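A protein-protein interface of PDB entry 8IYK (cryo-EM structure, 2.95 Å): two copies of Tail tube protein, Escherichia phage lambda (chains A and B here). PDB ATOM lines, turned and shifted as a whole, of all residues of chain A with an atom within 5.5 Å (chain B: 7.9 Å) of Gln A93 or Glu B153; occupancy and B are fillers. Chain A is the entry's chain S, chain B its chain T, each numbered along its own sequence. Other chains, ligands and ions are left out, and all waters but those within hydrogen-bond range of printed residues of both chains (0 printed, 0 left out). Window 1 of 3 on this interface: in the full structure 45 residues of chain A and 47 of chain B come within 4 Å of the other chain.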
ATOM      1  N   LEU A  39     -35.086 -15.781 -15.276  1.00  0.00           N
ATOM      2  CA  LEU A  39     -33.844 -16.267 -14.676  1.00  0.00           C
ATOM      3  C   LEU A  39     -32.725 -16.007 -15.678  1.00  0.00           C
ATOM      4  O   LEU A  39     -32.522 -16.786 -16.613  1.00  0.00           O
ATOM      5  CB  LEU A  39     -33.948 -17.746 -14.325  1.00  0.00           C
ATOM      6  CG  LEU A  39     -34.447 -18.093 -12.923  1.00  0.00           C
ATOM      7  CD1 LEU A  39     -34.829 -19.557 -12.853  1.00  0.00           C
ATOM      8  CD2 LEU A  39     -33.390 -17.764 -11.886  1.00  0.00           C
ATOM      9  N   LEU A  84     -26.721 -21.382 -13.639  1.00  0.00           N
ATOM     10  CA  LEU A  84     -26.644 -19.980 -14.021  1.00  0.00           C
ATOM     11  C   LEU A  84     -25.562 -19.300 -13.191  1.00  0.00           C
ATOM     12  O   LEU A  84     -24.922 -19.921 -12.343  1.00  0.00           O
ATOM     13  CB  LEU A  84     -27.992 -19.270 -13.841  1.00  0.00           C
ATOM     14  CG  LEU A  84     -28.789 -19.521 -12.563  1.00  0.00           C
ATOM     15  CD1 LEU A  84     -29.340 -18.213 -12.029  1.00  0.00           C
ATOM     16  CD2 LEU A  84     -29.915 -20.490 -12.831  1.00  0.00           C
ATOM     17  N   ALA A  85     -25.345 -18.015 -13.449  1.00  0.00           N
ATOM     18  CA  ALA A  85     -24.417 -17.251 -12.633  1.00  0.00           C
ATOM     19  C   ALA A  85     -25.010 -17.008 -11.249  1.00  0.00           C
ATOM     20  O   ALA A  85     -26.227 -17.036 -11.052  1.00  0.00           O
ATOM     21  CB  ALA A  85     -24.074 -15.924 -13.307  1.00  0.00           C
ATOM     22  N   TRP A  86     -24.132 -16.778 -10.277  1.00  0.00           N
ATOM     23  CA  TRP A  86     -24.553 -16.568  -8.895  1.00  0.00           C
ATOM     24  C   TRP A  86     -24.748 -15.076  -8.651  1.00  0.00           C
ATOM     25  O   TRP A  86     -23.777 -14.315  -8.588  1.00  0.00           O
ATOM     26  CB  TRP A  86     -23.535 -17.149  -7.918  1.00  0.00           C
ATOM     27  CG  TRP A  86     -24.072 -17.294  -6.531  1.00  0.00           C
ATOM     28  CD1 TRP A  86     -25.253 -17.868  -6.168  1.00  0.00           C
ATOM     29  CD2 TRP A  86     -23.453 -16.851  -5.317  1.00  0.00           C
ATOM     30  NE1 TRP A  86     -25.408 -17.815  -4.807  1.00  0.00           N
ATOM     31  CE2 TRP A  86     -24.316 -17.195  -4.261  1.00  0.00           C
ATOM     32  CE3 TRP A  86     -22.253 -16.199  -5.023  1.00  0.00           C
ATOM     33  CZ2 TRP A  86     -24.019 -16.909  -2.932  1.00  0.00           C
ATOM     34  CZ3 TRP A  86     -21.960 -15.918  -3.704  1.00  0.00           C
ATOM     35  CH2 TRP A  86     -22.839 -16.271  -2.675  1.00  0.00           C
ATOM     36  N   MET A  87     -26.006 -14.661  -8.512  1.00  0.00           N
ATOM     37  CA  MET A  87     -26.359 -13.301  -8.112  1.00  0.00           C
ATOM     38  C   MET A  87     -27.298 -13.423  -6.921  1.00  0.00           C
ATOM     39  O   MET A  87     -28.526 -13.412  -7.081  1.00  0.00           O
ATOM     40  CB  MET A  87     -27.000 -12.518  -9.256  1.00  0.00           C
ATOM     41  CG  MET A  87     -26.011 -11.986 -10.280  1.00  0.00           C
ATOM     42  SD  MET A  87     -26.519 -12.271 -11.985  1.00  0.00           S
ATOM     43  CE  MET A  87     -26.886 -14.018 -11.946  1.00  0.00           C
ATOM     44  N   PRO A  88     -26.754 -13.552  -5.709  1.00  0.00           N
ATOM     45  CA  PRO A  88     -27.607 -13.840  -4.544  1.00  0.00           C
ATOM     46  C   PRO A  88     -28.616 -12.753  -4.225  1.00  0.00           C
ATOM     47  O   PRO A  88     -29.631 -13.046  -3.582  1.00  0.00           O
ATOM     48  CB  PRO A  88     -26.592 -14.009  -3.405  1.00  0.00           C
ATOM     49  CG  PRO A  88     -25.394 -13.247  -3.851  1.00  0.00           C
ATOM     50  CD  PRO A  88     -25.338 -13.402  -5.340  1.00  0.00           C
ATOM     51  N   GLU A  90     -30.634 -10.849  -6.257  1.00  0.00           N
ATOM     52  CA  GLU A  90     -31.472 -10.501  -7.395  1.00  0.00           C
ATOM     53  C   GLU A  90     -32.705 -11.394  -7.414  1.00  0.00           C
ATOM     54  O   GLU A  90     -32.615 -12.599  -7.158  1.00  0.00           O
ATOM     55  CB  GLU A  90     -30.670 -10.603  -8.712  1.00  0.00           C
ATOM     56  CG  GLU A  90     -30.659 -11.964  -9.389  1.00  0.00           C
ATOM     57  CD  GLU A  90     -31.676 -12.076 -10.504  1.00  0.00           C
ATOM     58  OE1 GLU A  90     -32.254 -11.039 -10.890  1.00  0.00           O
ATOM     59  OE2 GLU A  90     -31.898 -13.201 -10.999  1.00  0.00           O
ATOM     60  N   GLN A  91     -33.859 -10.788  -7.679  1.00  0.00           N
ATOM     61  CA  GLN A  91     -35.111 -11.533  -7.702  1.00  0.00           C
ATOM     62  C   GLN A  91     -35.126 -12.539  -8.844  1.00  0.00           C
ATOM     63  O   GLN A  91     -34.565 -12.310  -9.917  1.00  0.00           O
ATOM     64  CB  GLN A  91     -36.306 -10.586  -7.820  1.00  0.00           C
ATOM     65  CG  GLN A  91     -36.361  -9.510  -6.752  1.00  0.00           C
ATOM     66  CD  GLN A  91     -36.043  -8.130  -7.286  1.00  0.00           C
ATOM     67  OE1 GLN A  91     -36.455  -7.120  -6.720  1.00  0.00           O
ATOM     68  NE2 GLN A  91     -35.293  -8.082  -8.381  1.00  0.00           N
ATOM     69  N   GLY A  92     -35.787 -13.664  -8.601  1.00  0.00           N
ATOM     70  CA  GLY A  92     -35.727 -14.788  -9.510  1.00  0.00           C
ATOM     71  C   GLY A  92     -34.786 -15.832  -8.954  1.00  0.00           C
ATOM     72  O   GLY A  92     -35.033 -17.036  -9.065  1.00  0.00           O
ATOM     73  N   GLN A  93     -33.698 -15.367  -8.341  1.00  0.00           N
ATOM     74  CA  GLN A  93     -32.777 -16.242  -7.631  1.00  0.00           C
ATOM     75  C   GLN A  93     -33.132 -16.353  -6.154  1.00  0.00           C
ATOM     76  O   GLN A  93     -33.053 -17.443  -5.580  1.00  0.00           O
ATOM     77  CB  GLN A  93     -31.343 -15.736  -7.795  1.00  0.00           C
ATOM     78  CG  GLN A  93     -30.629 -16.321  -8.997  1.00  0.00           C
ATOM     79  CD  GLN A  93     -29.130 -16.360  -8.822  1.00  0.00           C
ATOM     80  OE1 GLN A  93     -28.386 -15.845  -9.653  1.00  0.00           O
ATOM     81  NE2 GLN A  93     -28.676 -16.974  -7.738  1.00  0.00           N
ATOM     82  N   GLN A  94     -33.520 -15.241  -5.526  1.00  0.00           N
ATOM     83  CA  GLN A  94     -34.113 -15.322  -4.197  1.00  0.00           C
ATOM     84  C   GLN A  94     -35.433 -16.077  -4.246  1.00  0.00           C
ATOM     85  O   GLN A  94     -35.726 -16.902  -3.372  1.00  0.00           O
ATOM     86  CB  GLN A  94     -34.323 -13.922  -3.624  1.00  0.00           C
ATOM     87  CG  GLN A  94     -33.235 -12.932  -3.980  1.00  0.00           C
ATOM     88  CD  GLN A  94     -33.388 -11.619  -3.244  1.00  0.00           C
ATOM     89  OE1 GLN A  94     -33.641 -11.597  -2.041  1.00  0.00           O
ATOM     90  NE2 GLN A  94     -33.236 -10.515  -3.964  1.00  0.00           N
ATOM     91  N   ALA A  95     -36.243 -15.805  -5.272  1.00  0.00           N
ATOM     92  CA  ALA A  95     -37.470 -16.563  -5.469  1.00  0.00           C
ATOM     93  C   ALA A  95     -37.176 -18.031  -5.735  1.00  0.00           C
ATOM     94  O   ALA A  95     -37.988 -18.892  -5.398  1.00  0.00           O
ATOM     95  CB  ALA A  95     -38.280 -15.966  -6.619  1.00  0.00           C
ATOM     96  N   LEU A  96     -36.018 -18.336  -6.321  1.00  0.00           N
ATOM     97  CA  LEU A  96     -35.636 -19.731  -6.523  1.00  0.00           C
ATOM     98  C   LEU A  96     -35.368 -20.433  -5.195  1.00  0.00           C
ATOM     99  O   LEU A  96     -35.801 -21.573  -4.986  1.00  0.00           O
ATOM    100  CB  LEU A  96     -34.410 -19.799  -7.429  1.00  0.00           C
ATOM    101  CG  LEU A  96     -33.941 -21.175  -7.881  1.00  0.00           C
ATOM    102  CD1 LEU A  96     -34.958 -21.800  -8.817  1.00  0.00           C
ATOM    103  CD2 LEU A  96     -32.600 -21.036  -8.561  1.00  0.00           C
ATOM    104  N   LEU A  97     -34.656 -19.769  -4.282  1.00  0.00           N
ATOM    105  CA  LEU A  97     -34.428 -20.356  -2.966  1.00  0.00           C
ATOM    106  C   LEU A  97     -35.734 -20.483  -2.193  1.00  0.00           C
ATOM    107  O   LEU A  97     -35.940 -21.462  -1.467  1.00  0.00           O
ATOM    108  CB  LEU A  97     -33.414 -19.522  -2.186  1.00  0.00           C
ATOM    109  CG  LEU A  97     -31.996 -20.089  -2.115  1.00  0.00           C
ATOM    110  CD1 LEU A  97     -31.973 -21.367  -1.301  1.00  0.00           C
ATOM    111  CD2 LEU A  97     -31.439 -20.326  -3.508  1.00  0.00           C
ATOM    112  N   ALA A  98     -36.629 -19.503  -2.341  1.00  0.00           N
ATOM    113  CA  ALA A  98     -37.957 -19.631  -1.753  1.00  0.00           C
ATOM    114  C   ALA A  98     -38.701 -20.826  -2.338  1.00  0.00           C
ATOM    115  O   ALA A  98     -39.374 -21.563  -1.614  1.00  0.00           O
ATOM    116  CB  ALA A  98     -38.753 -18.344  -1.962  1.00  0.00           C
ATOM    117  N   ARG A 139     -24.472 -21.107  -9.766  1.00  0.00           N
ATOM    118  CA  ARG A 139     -25.516 -21.735  -8.970  1.00  0.00           C
ATOM    119  C   ARG A 139     -26.187 -22.795  -9.832  1.00  0.00           C
ATOM    120  O   ARG A 139     -26.665 -22.496 -10.932  1.00  0.00           O
ATOM    121  CB  ARG A 139     -26.532 -20.700  -8.485  1.00  0.00           C
ATOM    122  CG  ARG A 139     -27.916 -21.258  -8.231  1.00  0.00           C
ATOM    123  CD  ARG A 139     -27.976 -21.978  -6.898  1.00  0.00           C
ATOM    124  NE  ARG A 139     -28.004 -21.047  -5.777  1.00  0.00           N
ATOM    125  CZ  ARG A 139     -27.368 -21.237  -4.629  1.00  0.00           C
ATOM    126  NH1 ARG A 139     -26.630 -22.313  -4.419  1.00  0.00           N
ATOM    127  NH2 ARG A 139     -27.476 -20.324  -3.670  1.00  0.00           N
ATOM    128  N   PRO B   6     -23.822  -7.863  -5.115  1.00  0.00           N
ATOM    129  CA  PRO B   6     -24.558  -9.136  -5.163  1.00  0.00           C
ATOM    130  C   PRO B   6     -25.441  -9.291  -6.389  1.00  0.00           C
ATOM    131  O   PRO B   6     -25.844 -10.418  -6.697  1.00  0.00           O
ATOM    132  CB  PRO B   6     -25.395  -9.110  -3.877  1.00  0.00           C
ATOM    133  CG  PRO B   6     -25.498  -7.665  -3.521  1.00  0.00           C
ATOM    134  CD  PRO B   6     -24.206  -7.045  -3.954  1.00  0.00           C
ATOM    135  N   THR B   7     -25.759  -8.209  -7.093  1.00  0.00           N
ATOM    136  CA  THR B   7     -26.598  -8.283  -8.281  1.00  0.00           C
ATOM    137  C   THR B   7     -25.800  -8.539  -9.551  1.00  0.00           C
ATOM    138  O   THR B   7     -26.384  -8.556 -10.639  1.00  0.00           O
ATOM    139  CB  THR B   7     -27.413  -6.996  -8.439  1.00  0.00           C
ATOM    140  OG1 THR B   7     -26.528  -5.889  -8.646  1.00  0.00           O
ATOM    141  CG2 THR B   7     -28.247  -6.742  -7.197  1.00  0.00           C
ATOM    142  N   PRO B   9     -22.430 -11.071 -11.237  1.00  0.00           N
ATOM    143  CA  PRO B   9     -21.591 -12.245 -10.972  1.00  0.00           C
ATOM    144  C   PRO B   9     -20.212 -11.852 -10.462  1.00  0.00           C
ATOM    145  O   PRO B   9     -19.670 -10.801 -10.808  1.00  0.00           O
ATOM    146  CB  PRO B   9     -21.503 -12.941 -12.337  1.00  0.00           C
ATOM    147  CG  PRO B   9     -21.983 -11.933 -13.335  1.00  0.00           C
ATOM    148  CD  PRO B   9     -22.947 -11.060 -12.614  1.00  0.00           C
ATOM    149  N   THR B 116     -21.457 -11.078   0.949  1.00  0.00           N
ATOM    150  CA  THR B 116     -22.412 -12.047   1.459  1.00  0.00           C
ATOM    151  C   THR B 116     -21.670 -13.179   2.156  1.00  0.00           C
ATOM    152  O   THR B 116     -20.440 -13.266   2.117  1.00  0.00           O
ATOM    153  CB  THR B 116     -23.284 -12.597   0.326  1.00  0.00           C
ATOM    154  OG1 THR B 116     -22.445 -13.143  -0.697  1.00  0.00           O
ATOM    155  CG2 THR B 116     -24.133 -11.489  -0.270  1.00  0.00           C
ATOM    156  N   VAL B 117     -22.435 -14.055   2.799  1.00  0.00           N
ATOM    157  CA  VAL B 117     -21.855 -15.131   3.593  1.00  0.00           C
ATOM    158  C   VAL B 117     -22.890 -16.238   3.733  1.00  0.00           C
ATOM    159  O   VAL B 117     -24.076 -15.975   3.949  1.00  0.00           O
ATOM    160  CB  VAL B 117     -21.380 -14.607   4.969  1.00  0.00           C
ATOM    161  CG1 VAL B 117     -22.392 -13.630   5.540  1.00  0.00           C
ATOM    162  CG2 VAL B 117     -21.144 -15.753   5.931  1.00  0.00           C
ATOM    163  N   ASP B 118     -22.430 -17.479   3.603  1.00  0.00           N
ATOM    164  CA  ASP B 118     -23.250 -18.661   3.839  1.00  0.00           C
ATOM    165  C   ASP B 118     -22.831 -19.292   5.158  1.00  0.00           C
ATOM    166  O   ASP B 118     -21.638 -19.466   5.407  1.00  0.00           O
ATOM    167  CB  ASP B 118     -23.100 -19.677   2.704  1.00  0.00           C
ATOM    168  CG  ASP B 118     -23.950 -19.337   1.500  1.00  0.00           C
ATOM    169  OD1 ASP B 118     -24.647 -18.303   1.536  1.00  0.00           O
ATOM    170  OD2 ASP B 118     -23.925 -20.108   0.517  1.00  0.00           O
ATOM    171  N   ARG B 148     -31.147 -26.776   9.174  1.00  0.00           N
ATOM    172  CA  ARG B 148     -31.403 -25.840   8.087  1.00  0.00           C
ATOM    173  C   ARG B 148     -30.262 -24.846   7.975  1.00  0.00           C
ATOM    174  O   ARG B 148     -29.908 -24.206   8.975  1.00  0.00           O
ATOM    175  CB  ARG B 148     -32.714 -25.094   8.317  1.00  0.00           C
ATOM    176  CG  ARG B 148     -32.910 -23.903   7.396  1.00  0.00           C
ATOM    177  CD  ARG B 148     -34.121 -23.083   7.802  1.00  0.00           C
ATOM    178  NE  ARG B 148     -34.695 -22.349   6.679  1.00  0.00           N
ATOM    179  CZ  ARG B 148     -34.156 -21.268   6.132  1.00  0.00           C
ATOM    180  NH1 ARG B 148     -33.026 -20.752   6.585  1.00  0.00           N
ATOM    181  NH2 ARG B 148     -34.773 -20.683   5.109  1.00  0.00           N
ATOM    182  N   SER B 150     -28.236 -21.346   6.498  1.00  0.00           N
ATOM    183  CA  SER B 150     -28.569 -19.936   6.310  1.00  0.00           C
ATOM    184  C   SER B 150     -27.850 -19.432   5.060  1.00  0.00           C
ATOM    185  O   SER B 150     -26.718 -18.952   5.128  1.00  0.00           O
ATOM    186  CB  SER B 150     -28.191 -19.125   7.542  1.00  0.00           C
ATOM    187  OG  SER B 150     -27.990 -17.764   7.213  1.00  0.00           O
ATOM    188  N   MET B 151     -28.523 -19.539   3.917  1.00  0.00           N
ATOM    189  CA  MET B 151     -27.973 -19.067   2.656  1.00  0.00           C
ATOM    190  C   MET B 151     -27.836 -17.548   2.643  1.00  0.00           C
ATOM    191  O   MET B 151     -28.439 -16.830   3.443  1.00  0.00           O
ATOM    192  CB  MET B 151     -28.854 -19.508   1.485  1.00  0.00           C
ATOM    193  CG  MET B 151     -28.763 -20.975   1.036  1.00  0.00           C
ATOM    194  SD  MET B 151     -27.142 -21.786   1.017  1.00  0.00           S
ATOM    195  CE  MET B 151     -26.888 -22.262   2.723  1.00  0.00           C
ATOM    196  N   ALA B 152     -27.020 -17.062   1.704  1.00  0.00           N
ATOM    197  CA  ALA B 152     -26.859 -15.626   1.517  1.00  0.00           C
ATOM    198  C   ALA B 152     -28.131 -14.965   1.009  1.00  0.00           C
ATOM    199  O   ALA B 152     -28.254 -13.739   1.097  1.00  0.00           O
ATOM    200  CB  ALA B 152     -25.709 -15.346   0.550  1.00  0.00           C
ATOM    201  N   GLU B 153     -29.071 -15.744   0.472  1.00  0.00           N
ATOM    202  CA  GLU B 153     -30.355 -15.192   0.063  1.00  0.00           C
ATOM    203  C   GLU B 153     -31.259 -14.908   1.253  1.00  0.00           C
ATOM    204  O   GLU B 153     -32.253 -14.191   1.103  1.00  0.00           O
ATOM    205  CB  GLU B 153     -31.054 -16.151  -0.902  1.00  0.00           C
ATOM    206  CG  GLU B 153     -30.572 -16.059  -2.340  1.00  0.00           C
ATOM    207  CD  GLU B 153     -29.424 -17.004  -2.636  1.00  0.00           C
ATOM    208  OE1 GLU B 153     -28.740 -17.431  -1.682  1.00  0.00           O
ATOM    209  OE2 GLU B 153     -29.206 -17.320  -3.822  1.00  0.00           O
ATOM    210  N   ASP B 154     -30.937 -15.455   2.427  1.00  0.00           N
ATOM    211  CA  ASP B 154     -31.775 -15.244   3.602  1.00  0.00           C
ATOM    212  C   ASP B 154     -31.701 -13.804   4.091  1.00  0.00           C
ATOM    213  O   ASP B 154     -32.717 -13.227   4.493  1.00  0.00           O
ATOM    214  CB  ASP B 154     -31.364 -16.207   4.715  1.00  0.00           C
ATOM    215  CG  ASP B 154     -32.009 -17.568   4.574  1.00  0.00           C
ATOM    216  OD1 ASP B 154     -32.710 -17.792   3.566  1.00  0.00           O
ATOM    217  OD2 ASP B 154     -31.814 -18.416   5.470  1.00  0.00           O
ATOM    218  N   ARG B 155     -30.511 -13.207   4.067  1.00  0.00           N
ATOM    219  CA  ARG B 155     -30.303 -11.867   4.595  1.00  0.00           C
ATOM    220  C   ARG B 155     -30.272 -10.797   3.512  1.00  0.00           C
ATOM    221  O   ARG B 155     -29.890  -9.656   3.795  1.00  0.00           O
ATOM    222  CB  ARG B 155     -29.018 -11.819   5.426  1.00  0.00           C
ATOM    223  CG  ARG B 155     -27.741 -11.919   4.619  1.00  0.00           C
ATOM    224  CD  ARG B 155     -26.605 -12.416   5.491  1.00  0.00           C
ATOM    225  NE  ARG B 155     -27.034 -13.497   6.369  1.00  0.00           N
ATOM    226  CZ  ARG B 155     -26.710 -14.772   6.207  1.00  0.00           C
ATOM    227  NH1 ARG B 155     -25.950 -15.169   5.200  1.00  0.00           N
ATOM    228  NH2 ARG B 155     -27.156 -15.669   7.079  1.00  0.00           N
ATOM    229  N   SER B 156     -30.662 -11.130   2.287  1.00  0.00           N
ATOM    230  CA  SER B 156     -30.816 -10.111   1.264  1.00  0.00           C
ATOM    231  C   SER B 156     -32.062  -9.273   1.540  1.00  0.00           C
ATOM    232  O   SER B 156     -33.002  -9.709   2.210  1.00  0.00           O
ATOM    233  CB  SER B 156     -30.901 -10.747  -0.124  1.00  0.00           C
ATOM    234  OG  SER B 156     -32.175 -11.327  -0.339  1.00  0.00           O
ATOM    235  N   THR B 157     -32.060  -8.051   1.012  1.00  0.00           N
ATOM    236  CA  THR B 157     -33.143  -7.103   1.226  1.00  0.00           C
ATOM    237  C   THR B 157     -33.680  -6.611  -0.110  1.00  0.00           C
ATOM    238  O   THR B 157     -32.912  -6.342  -1.039  1.00  0.00           O
ATOM    239  CB  THR B 157     -32.678  -5.910   2.067  1.00  0.00           C
ATOM    240  OG1 THR B 157     -31.381  -5.488   1.628  1.00  0.00           O
ATOM    241  CG2 THR B 157     -32.613  -6.290   3.538  1.00  0.00           C
ATOM    242  N   VAL B 158     -35.003  -6.493  -0.197  1.00  0.00           N
ATOM    243  CA  VAL B 158     -35.686  -6.016  -1.394  1.00  0.00           C
ATOM    244  C   VAL B 158     -36.492  -4.775  -1.031  1.00  0.00           C
ATOM    245  O   VAL B 158     -37.028  -4.673   0.078  1.00  0.00           O
ATOM    246  CB  VAL B 158     -36.587  -7.106  -2.015  1.00  0.00           C
ATOM    247  CG1 VAL B 158     -35.785  -8.372  -2.270  1.00  0.00           C
ATOM    248  CG2 VAL B 158     -37.777  -7.410  -1.114  1.00  0.00           C
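The side-chain amide oxygen (OE1) of Gln A93 sits at hydrogen-bond distance from the backbone NH (N) of Met A87, at 2.9 Å. The backbone carbonyl oxygen (O) of Met B151 is in hydrogen-bond range of the guanidinium group (NH1) of Arg B155 (3.5 Å). The side-chain amide nitrogen (NE2) of Gln A94 lies close to the backbone NH (N) of Glu A90. O of Ala A85 sits close to OE1 of Gln A93 (2.8 Å). The side-chain hydroxyl (OG) of Ser B156 sits at hydrogen-bond distance from the backbone carbonyl oxygen (O) of Glu B153 (3.2 Å). The backbone carbonyl oxygen (O) of Leu A84 sits at hydrogen-bond distance from the backbone NH (N) of Arg A139 (2.9 Å).
The guanidinium group (NH2) of Arg A139 is in salt-bridge range of the side-chain carboxylate (OE2) of Glu B153, at 3.5 Å. The side-chain amide oxygen (OE1) of Gln A94 lies close to the side-chain hydroxyl (OG) of Ser B156 (2.3 Å). The backbone nitrogen of Pro A88 sits close to the backbone carbonyl oxygen of Pro B6, at 3.4 Å.
Among the printed residues, pairs that only touch across the chains: Met A87 with Pro B6, Pro A88 with Glu B153, Met A87 with Thr B7, Trp A86 with Thr B116, Gln A94 with Val B158, Leu A97 with Glu B153, Met A87 with Pro B9, Trp A86 with Pro B9, Trp A86 with Glu B153, Gln A93 with Glu B153 and Leu A97 with Met B151.
No position is printed for both chains.
Gln A93 touches just one residue of chain B: Glu B153 (3.97 Å). Glu B153 touches five residues of chain A. No residue of chain B comes within 4 Å of Gly A92. Printed residues of chain B within 4 Å of Trp A86: Pro B9, Thr B116 and Glu B153. Of the printed residues of chain A, Val B158 touches Gln A94 (3.7 Å). Of the printed residues of chain A, Ser B156 touches Gln A94. Printed residues of chain A within 4 Å of Pro B9: Trp A86 and Met A87. Leu A96 touches none of the printed residues of chain B. The nearest residue of chain B that does not touch Gln A93 is Pro B6 (6.7 Å). The nearest printed residue of chain A that does not touch Met B151 is Arg A139 (4.9 Å).
Of the 16 printed residues of chain B, 8 touch a printed residue of chain A. Among the printed residues, 14 pairs touch across the chains. Among the printed residues, Asp or Glu carboxylates within 4 Å of a Lys or Arg side-chain nitrogen of the other chain: Arg A139 with Glu B153 (3.5 Å).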
